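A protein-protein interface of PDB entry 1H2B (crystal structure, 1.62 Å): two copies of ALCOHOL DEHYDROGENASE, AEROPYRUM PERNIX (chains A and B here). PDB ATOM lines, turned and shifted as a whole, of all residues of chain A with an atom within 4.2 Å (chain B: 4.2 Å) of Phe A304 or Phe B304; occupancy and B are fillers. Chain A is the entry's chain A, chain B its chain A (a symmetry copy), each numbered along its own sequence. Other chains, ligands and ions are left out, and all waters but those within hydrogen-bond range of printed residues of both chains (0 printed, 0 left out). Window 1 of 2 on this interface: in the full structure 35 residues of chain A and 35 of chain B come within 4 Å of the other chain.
Phe A304 touches just these residues of chain B: Leu B290 (3.8 Å), Ser B303 (3.2 Å) and Phe B304 (2.8 Å).
Of the printed residues of chain B, Ser A303 touches Phe B304 and Glu B305.
Printed residues of chain A within 4 Å of Phe B292: Leu A290 (2.8 Å).
Printed residues of chain A within 4 Å of Leu B290: Leu A290, Phe A292 and Phe A304.
Of the printed residues of chain B, Phe A292 touches Leu B290 (2.8 Å).
Leu B275 touches none of the printed residues of chain A.
Val A297 touches none of the printed residues of chain B.
The nearest printed residue of chain A that does not touch Phe B304 is Glu A305 (5.0 Å).
The nearest printed residue of chain A that does not touch Glu B305 is Val A297 (4.6 Å).
Among the printed residues, pairs that only touch across the chains: Leu A290 with Phe B304 (3.8 Å), Ser A303 with Phe B304 (3.2 Å), Ser A303 with Glu B305 (3.9 Å), Phe A304 with Leu B290 (3.8 Å), Phe A304 with Ser B303 (3.2 Å) and Glu A305 with Ser B303 (3.9 Å).
Leu A290 touches Phe B292, and with the chains exchanged Phe A292 touches Leu B290.
Leu A290 touches Phe B304, and with the chains exchanged Phe A304 touches Leu B290.
Ser A303 touches Phe B304, and with the chains exchanged Phe A304 touches Ser B303.
Ser A303 touches Glu B305, and with the chains exchanged Glu A305 touches Ser B303.
Of the 10 pairs that touch across the chains among the printed residues, 10 have their exchanged pair printed and touching as well.
O of Ser A303 sits at hydrogen-bond distance from N of Leu A281, at 2.9 Å.
O of Leu A281 lies within hydrogen-bond range of N of Glu A305.
OE2 of Glu A305 is in hydrogen-bond range of OG of Ser A303, 2.7 Å away.
The backbone carbonyl oxygen (O) of Leu B281 is in hydrogen-bond range of the backbone NH (N) of Glu B305, 2.7 Å away.
The backbone carbonyl oxygen of Glu B305 is in hydrogen-bond range of the backbone NH of Ile B283 (2.8 Å).
The side-chain carboxylate (OE2) of Glu B305 lies within hydrogen-bond range of the side-chain hydroxyl (OG) of Ser B303, 2.7 Å away.
Of the 10 printed residues of chain B, 5 touch a printed residue of chain A.
The backbone NH (N) of Leu A290 is in hydrogen-bond range of the backbone carbonyl oxygen (O) of Phe B292, 2.8 Å away.
O of Phe A292 lies within hydrogen-bond range of N of Leu B290 (2.8 Å).
The backbone NH of Phe B304 lies within hydrogen-bond range of the backbone carbonyl oxygen of Phe A304 (2.8 Å).
O of Leu B290 lies close to O of Leu A290, at 3.3 Å.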
ATOM      1  N   PRO A 272       9.923 -25.874   5.719  1.00  0.00           N
ATOM      2  CA  PRO A 272       9.525 -24.517   5.283  1.00  0.00           C
ATOM      3  C   PRO A 272      10.572 -23.822   4.412  1.00  0.00           C
ATOM      4  O   PRO A 272      10.255 -22.965   3.611  1.00  0.00           O
ATOM      5  CB  PRO A 272       9.338 -23.746   6.613  1.00  0.00           C
ATOM      6  CG  PRO A 272       9.156 -24.794   7.634  1.00  0.00           C
ATOM      7  CD  PRO A 272       9.943 -26.016   7.189  1.00  0.00           C
ATOM      8  N   LEU A 275      10.524 -24.052   0.416  1.00  0.00           N
ATOM      9  CA  LEU A 275       9.504 -23.361  -0.376  1.00  0.00           C
ATOM     10  C   LEU A 275      10.050 -22.186  -1.168  1.00  0.00           C
ATOM     11  O   LEU A 275      10.834 -21.351  -0.673  1.00  0.00           O
ATOM     12  CB  LEU A 275       8.395 -22.762   0.531  1.00  0.00           C
ATOM     13  CG  LEU A 275       7.694 -23.771   1.447  1.00  0.00           C
ATOM     14  CD1 LEU A 275       6.631 -23.092   2.360  1.00  0.00           C
ATOM     15  CD2 LEU A 275       7.010 -24.885   0.623  1.00  0.00           C
ATOM     16  N   LEU A 281       3.455 -25.346   2.161  1.00  0.00           N
ATOM     17  CA  LEU A 281       3.859 -26.565   2.869  1.00  0.00           C
ATOM     18  C   LEU A 281       2.603 -27.207   3.414  1.00  0.00           C
ATOM     19  O   LEU A 281       1.860 -26.611   4.208  1.00  0.00           O
ATOM     20  CB  LEU A 281       4.766 -26.191   4.053  1.00  0.00           C
ATOM     21  CG  LEU A 281       5.139 -27.293   5.040  1.00  0.00           C
ATOM     22  CD1 LEU A 281       5.782 -28.536   4.401  1.00  0.00           C
ATOM     23  CD2 LEU A 281       6.063 -26.668   6.119  1.00  0.00           C
ATOM     24  N   ILE A 283       1.227 -29.804   5.774  1.00  0.00           N
ATOM     25  CA  ILE A 283       1.679 -30.521   6.954  1.00  0.00           C
ATOM     26  C   ILE A 283       0.745 -31.686   7.252  1.00  0.00           C
ATOM     27  O   ILE A 283      -0.460 -31.513   7.536  1.00  0.00           O
ATOM     28  CB  ILE A 283       1.746 -29.533   8.147  1.00  0.00           C
ATOM     29  CG1 ILE A 283       2.829 -28.495   7.858  1.00  0.00           C
ATOM     30  CG2 ILE A 283       2.007 -30.311   9.430  1.00  0.00           C
ATOM     31  CD1 ILE A 283       2.851 -27.307   8.858  1.00  0.00           C
ATOM     32  N   LEU A 290       6.220 -26.321  14.745  1.00  0.00           N
ATOM     33  CA  LEU A 290       6.535 -25.416  13.648  1.00  0.00           C
ATOM     34  C   LEU A 290       7.151 -24.119  14.184  1.00  0.00           C
ATOM     35  O   LEU A 290       6.598 -23.559  15.130  1.00  0.00           O
ATOM     36  CB  LEU A 290       5.239 -25.146  12.840  1.00  0.00           C
ATOM     37  CG  LEU A 290       5.309 -24.184  11.649  1.00  0.00           C
ATOM     38  CD1 LEU A 290       6.204 -24.686  10.501  1.00  0.00           C
ATOM     39  CD2 LEU A 290       3.881 -24.009  11.141  1.00  0.00           C
ATOM     40  N   PHE A 292       9.171 -20.614  12.577  1.00  0.00           N
ATOM     41  CA  PHE A 292       9.561 -20.004  11.323  1.00  0.00           C
ATOM     42  C   PHE A 292       9.344 -18.499  11.455  1.00  0.00           C
ATOM     43  O   PHE A 292       8.314 -18.081  12.000  1.00  0.00           O
ATOM     44  CB  PHE A 292       8.753 -20.597  10.181  1.00  0.00           C
ATOM     45  CG  PHE A 292       9.294 -20.293   8.829  1.00  0.00           C
ATOM     46  CD1 PHE A 292      10.441 -20.923   8.353  1.00  0.00           C
ATOM     47  CD2 PHE A 292       8.671 -19.371   8.007  1.00  0.00           C
ATOM     48  CE1 PHE A 292      10.940 -20.638   7.081  1.00  0.00           C
ATOM     49  CE2 PHE A 292       9.162 -19.088   6.745  1.00  0.00           C
ATOM     50  CZ  PHE A 292      10.287 -19.723   6.265  1.00  0.00           C
ATOM     51  N   VAL A 297       7.684 -15.545   6.244  1.00  0.00           N
ATOM     52  CA  VAL A 297       6.321 -15.914   5.847  1.00  0.00           C
ATOM     53  C   VAL A 297       5.791 -14.851   4.878  1.00  0.00           C
ATOM     54  O   VAL A 297       5.244 -15.199   3.828  1.00  0.00           O
ATOM     55  CB  VAL A 297       5.381 -16.027   7.069  1.00  0.00           C
ATOM     56  CG1 VAL A 297       3.913 -16.219   6.644  1.00  0.00           C
ATOM     57  CG2 VAL A 297       5.791 -17.230   7.924  1.00  0.00           C
ATOM     58  N   SER A 303       2.629 -20.324   2.734  1.00  0.00           N
ATOM     59  CA  SER A 303       1.603 -20.800   3.635  1.00  0.00           C
ATOM     60  C   SER A 303       1.984 -22.169   4.163  1.00  0.00           C
ATOM     61  O   SER A 303       2.732 -22.936   3.520  1.00  0.00           O
ATOM     62  CB  SER A 303       0.246 -20.873   2.936  1.00  0.00           C
ATOM     63  OG  SER A 303       0.311 -21.748   1.838  1.00  0.00           O
ATOM     64  N   PHE A 304       1.417 -22.481   5.310  1.00  0.00           N
ATOM     65  CA  PHE A 304       1.613 -23.748   5.984  1.00  0.00           C
ATOM     66  C   PHE A 304       0.224 -24.274   6.261  1.00  0.00           C
ATOM     67  O   PHE A 304      -0.573 -23.603   6.927  1.00  0.00           O
ATOM     68  CB  PHE A 304       2.354 -23.554   7.326  1.00  0.00           C
ATOM     69  CG  PHE A 304       3.658 -22.811   7.218  1.00  0.00           C
ATOM     70  CD1 PHE A 304       3.979 -21.833   8.133  1.00  0.00           C
ATOM     71  CD2 PHE A 304       4.559 -23.076   6.207  1.00  0.00           C
ATOM     72  CE1 PHE A 304       5.187 -21.142   8.039  1.00  0.00           C
ATOM     73  CE2 PHE A 304       5.758 -22.383   6.091  1.00  0.00           C
ATOM     74  CZ  PHE A 304       6.066 -21.410   6.986  1.00  0.00           C
ATOM     75  N   GLU A 305      -0.099 -25.457   5.724  1.00  0.00           N
ATOM     76  CA  GLU A 305      -1.507 -25.898   5.659  1.00  0.00           C
ATOM     77  C   GLU A 305      -1.613 -27.308   6.200  1.00  0.00           C
ATOM     78  O   GLU A 305      -1.079 -28.234   5.574  1.00  0.00           O
ATOM     79  CB  GLU A 305      -2.021 -25.879   4.201  1.00  0.00           C
ATOM     80  CG  GLU A 305      -1.893 -24.475   3.574  1.00  0.00           C
ATOM     81  CD  GLU A 305      -2.205 -24.422   2.102  1.00  0.00           C
ATOM     82  OE1 GLU A 305      -3.127 -25.115   1.665  1.00  0.00           O
ATOM     83  OE2 GLU A 305      -1.528 -23.653   1.420  1.00  0.00           O
ATOM     84  N   PRO B 272      -2.757 -18.032  16.536  1.00  0.00           N
ATOM     85  CA  PRO B 272      -3.127 -19.387  16.071  1.00  0.00           C
ATOM     86  C   PRO B 272      -4.153 -20.082  16.966  1.00  0.00           C
ATOM     87  O   PRO B 272      -4.895 -20.938  16.525  1.00  0.00           O
ATOM     88  CB  PRO B 272      -1.784 -20.160  16.097  1.00  0.00           C
ATOM     89  CG  PRO B 272      -0.747 -19.113  16.081  1.00  0.00           C
ATOM     90  CD  PRO B 272      -1.309 -17.892  16.789  1.00  0.00           C
ATOM     91  N   LEU B 275      -8.091 -19.846  16.286  1.00  0.00           N
ATOM     92  CA  LEU B 275      -8.712 -20.535  15.152  1.00  0.00           C
ATOM     93  C   LEU B 275      -9.582 -21.710  15.564  1.00  0.00           C
ATOM     94  O   LEU B 275      -9.219 -22.546  16.415  1.00  0.00           O
ATOM     95  CB  LEU B 275      -7.642 -21.133  14.200  1.00  0.00           C
ATOM     96  CG  LEU B 275      -6.625 -20.125  13.654  1.00  0.00           C
ATOM     97  CD1 LEU B 275      -5.555 -20.805  12.748  1.00  0.00           C
ATOM     98  CD2 LEU B 275      -7.328 -19.009  12.850  1.00  0.00           C
ATOM     99  N   LEU B 281      -5.245 -18.546   9.584  1.00  0.00           N
ATOM    100  CA  LEU B 281      -4.609 -17.328  10.098  1.00  0.00           C
ATOM    101  C   LEU B 281      -3.871 -16.686   8.945  1.00  0.00           C
ATOM    102  O   LEU B 281      -2.970 -17.282   8.337  1.00  0.00           O
ATOM    103  CB  LEU B 281      -3.584 -17.705  11.180  1.00  0.00           C
ATOM    104  CG  LEU B 281      -2.668 -16.605  11.707  1.00  0.00           C
ATOM    105  CD1 LEU B 281      -3.399 -15.363  12.242  1.00  0.00           C
ATOM    106  CD2 LEU B 281      -1.750 -17.233  12.789  1.00  0.00           C
ATOM    107  N   ILE B 283      -1.320 -14.091   7.965  1.00  0.00           N
ATOM    108  CA  ILE B 283      -0.225 -13.376   8.599  1.00  0.00           C
ATOM    109  C   ILE B 283       0.218 -12.210   7.726  1.00  0.00           C
ATOM    110  O   ILE B 283       0.690 -12.382   6.580  1.00  0.00           O
ATOM    111  CB  ILE B 283       0.941 -14.366   8.853  1.00  0.00           C
ATOM    112  CG1 ILE B 283       0.482 -15.404   9.875  1.00  0.00           C
ATOM    113  CG2 ILE B 283       2.167 -13.590   9.315  1.00  0.00           C
ATOM    114  CD1 ILE B 283       1.465 -16.594  10.053  1.00  0.00           C
ATOM    115  N   LEU B 290       6.742 -17.594  14.311  1.00  0.00           N
ATOM    116  CA  LEU B 290       5.608 -18.497  14.448  1.00  0.00           C
ATOM    117  C   LEU B 290       6.038 -19.795  15.138  1.00  0.00           C
ATOM    118  O   LEU B 290       7.059 -20.356  14.742  1.00  0.00           O
ATOM    119  CB  LEU B 290       5.015 -18.764  13.039  1.00  0.00           C
ATOM    120  CG  LEU B 290       3.827 -19.724  12.918  1.00  0.00           C
ATOM    121  CD1 LEU B 290       2.552 -19.222  13.620  1.00  0.00           C
ATOM    122  CD2 LEU B 290       3.552 -19.897  11.427  1.00  0.00           C
ATOM    123  N   PHE B 292       4.126 -23.301  16.872  1.00  0.00           N
ATOM    124  CA  PHE B 292       2.826 -23.910  17.059  1.00  0.00           C
ATOM    125  C   PHE B 292       2.989 -25.414  16.863  1.00  0.00           C
ATOM    126  O   PHE B 292       3.689 -25.831  15.931  1.00  0.00           O
ATOM    127  CB  PHE B 292       1.827 -23.313  16.080  1.00  0.00           C
ATOM    128  CG  PHE B 292       0.406 -23.616  16.400  1.00  0.00           C
ATOM    129  CD1 PHE B 292      -0.245 -22.987  17.458  1.00  0.00           C
ATOM    130  CD2 PHE B 292      -0.308 -24.537  15.653  1.00  0.00           C
ATOM    131  CE1 PHE B 292      -1.581 -23.271  17.748  1.00  0.00           C
ATOM    132  CE2 PHE B 292      -1.632 -24.818  15.937  1.00  0.00           C
ATOM    133  CZ  PHE B 292      -2.284 -24.184  16.972  1.00  0.00           C
ATOM    134  N   VAL B 297      -1.898 -28.358  14.393  1.00  0.00           N
ATOM    135  CA  VAL B 297      -2.073 -27.987  12.985  1.00  0.00           C
ATOM    136  C   VAL B 297      -2.947 -29.048  12.306  1.00  0.00           C
ATOM    137  O   VAL B 297      -3.897 -28.698  11.600  1.00  0.00           O
ATOM    138  CB  VAL B 297      -0.717 -27.875  12.250  1.00  0.00           C
ATOM    139  CG1 VAL B 297      -0.904 -27.680  10.734  1.00  0.00           C
ATOM    140  CG2 VAL B 297       0.063 -26.674  12.792  1.00  0.00           C
ATOM    141  N   SER B 303      -4.556 -23.568   8.852  1.00  0.00           N
ATOM    142  CA  SER B 303      -3.502 -23.091   7.983  1.00  0.00           C
ATOM    143  C   SER B 303      -3.039 -21.724   8.445  1.00  0.00           C
ATOM    144  O   SER B 303      -3.792 -20.957   9.082  1.00  0.00           O
ATOM    145  CB  SER B 303      -3.978 -23.016   6.533  1.00  0.00           C
ATOM    146  OG  SER B 303      -5.071 -22.139   6.424  1.00  0.00           O
ATOM    147  N   PHE B 304      -1.817 -21.413   8.068  1.00  0.00           N
ATOM    148  CA  PHE B 304      -1.181 -20.148   8.370  1.00  0.00           C
ATOM    149  C   PHE B 304      -0.687 -19.620   7.043  1.00  0.00           C
ATOM    150  O   PHE B 304       0.097 -20.291   6.361  1.00  0.00           O
ATOM    151  CB  PHE B 304       0.026 -20.344   9.314  1.00  0.00           C
ATOM    152  CG  PHE B 304      -0.288 -21.089  10.583  1.00  0.00           C
ATOM    153  CD1 PHE B 304       0.564 -22.068  11.044  1.00  0.00           C
ATOM    154  CD2 PHE B 304      -1.429 -20.823  11.313  1.00  0.00           C
ATOM    155  CE1 PHE B 304       0.278 -22.761  12.221  1.00  0.00           C
ATOM    156  CE2 PHE B 304      -1.735 -21.518  12.478  1.00  0.00           C
ATOM    157  CZ  PHE B 304      -0.900 -22.492  12.921  1.00  0.00           C
ATOM    158  N   GLU B 305      -1.163 -18.435   6.641  1.00  0.00           N
ATOM    159  CA  GLU B 305      -1.004 -17.993   5.241  1.00  0.00           C
ATOM    160  C   GLU B 305      -0.451 -16.584   5.224  1.00  0.00           C
ATOM    161  O   GLU B 305      -1.153 -15.657   5.654  1.00  0.00           O
ATOM    162  CB  GLU B 305      -2.362 -18.009   4.502  1.00  0.00           C
ATOM    163  CG  GLU B 305      -3.004 -19.412   4.527  1.00  0.00           C
ATOM    164  CD  GLU B 305      -4.407 -19.462   3.985  1.00  0.00           C
ATOM    165  OE1 GLU B 305      -4.692 -18.768   3.007  1.00  0.00           O
ATOM    166  OE2 GLU B 305      -5.190 -20.231   4.545  1.00  0.00           O
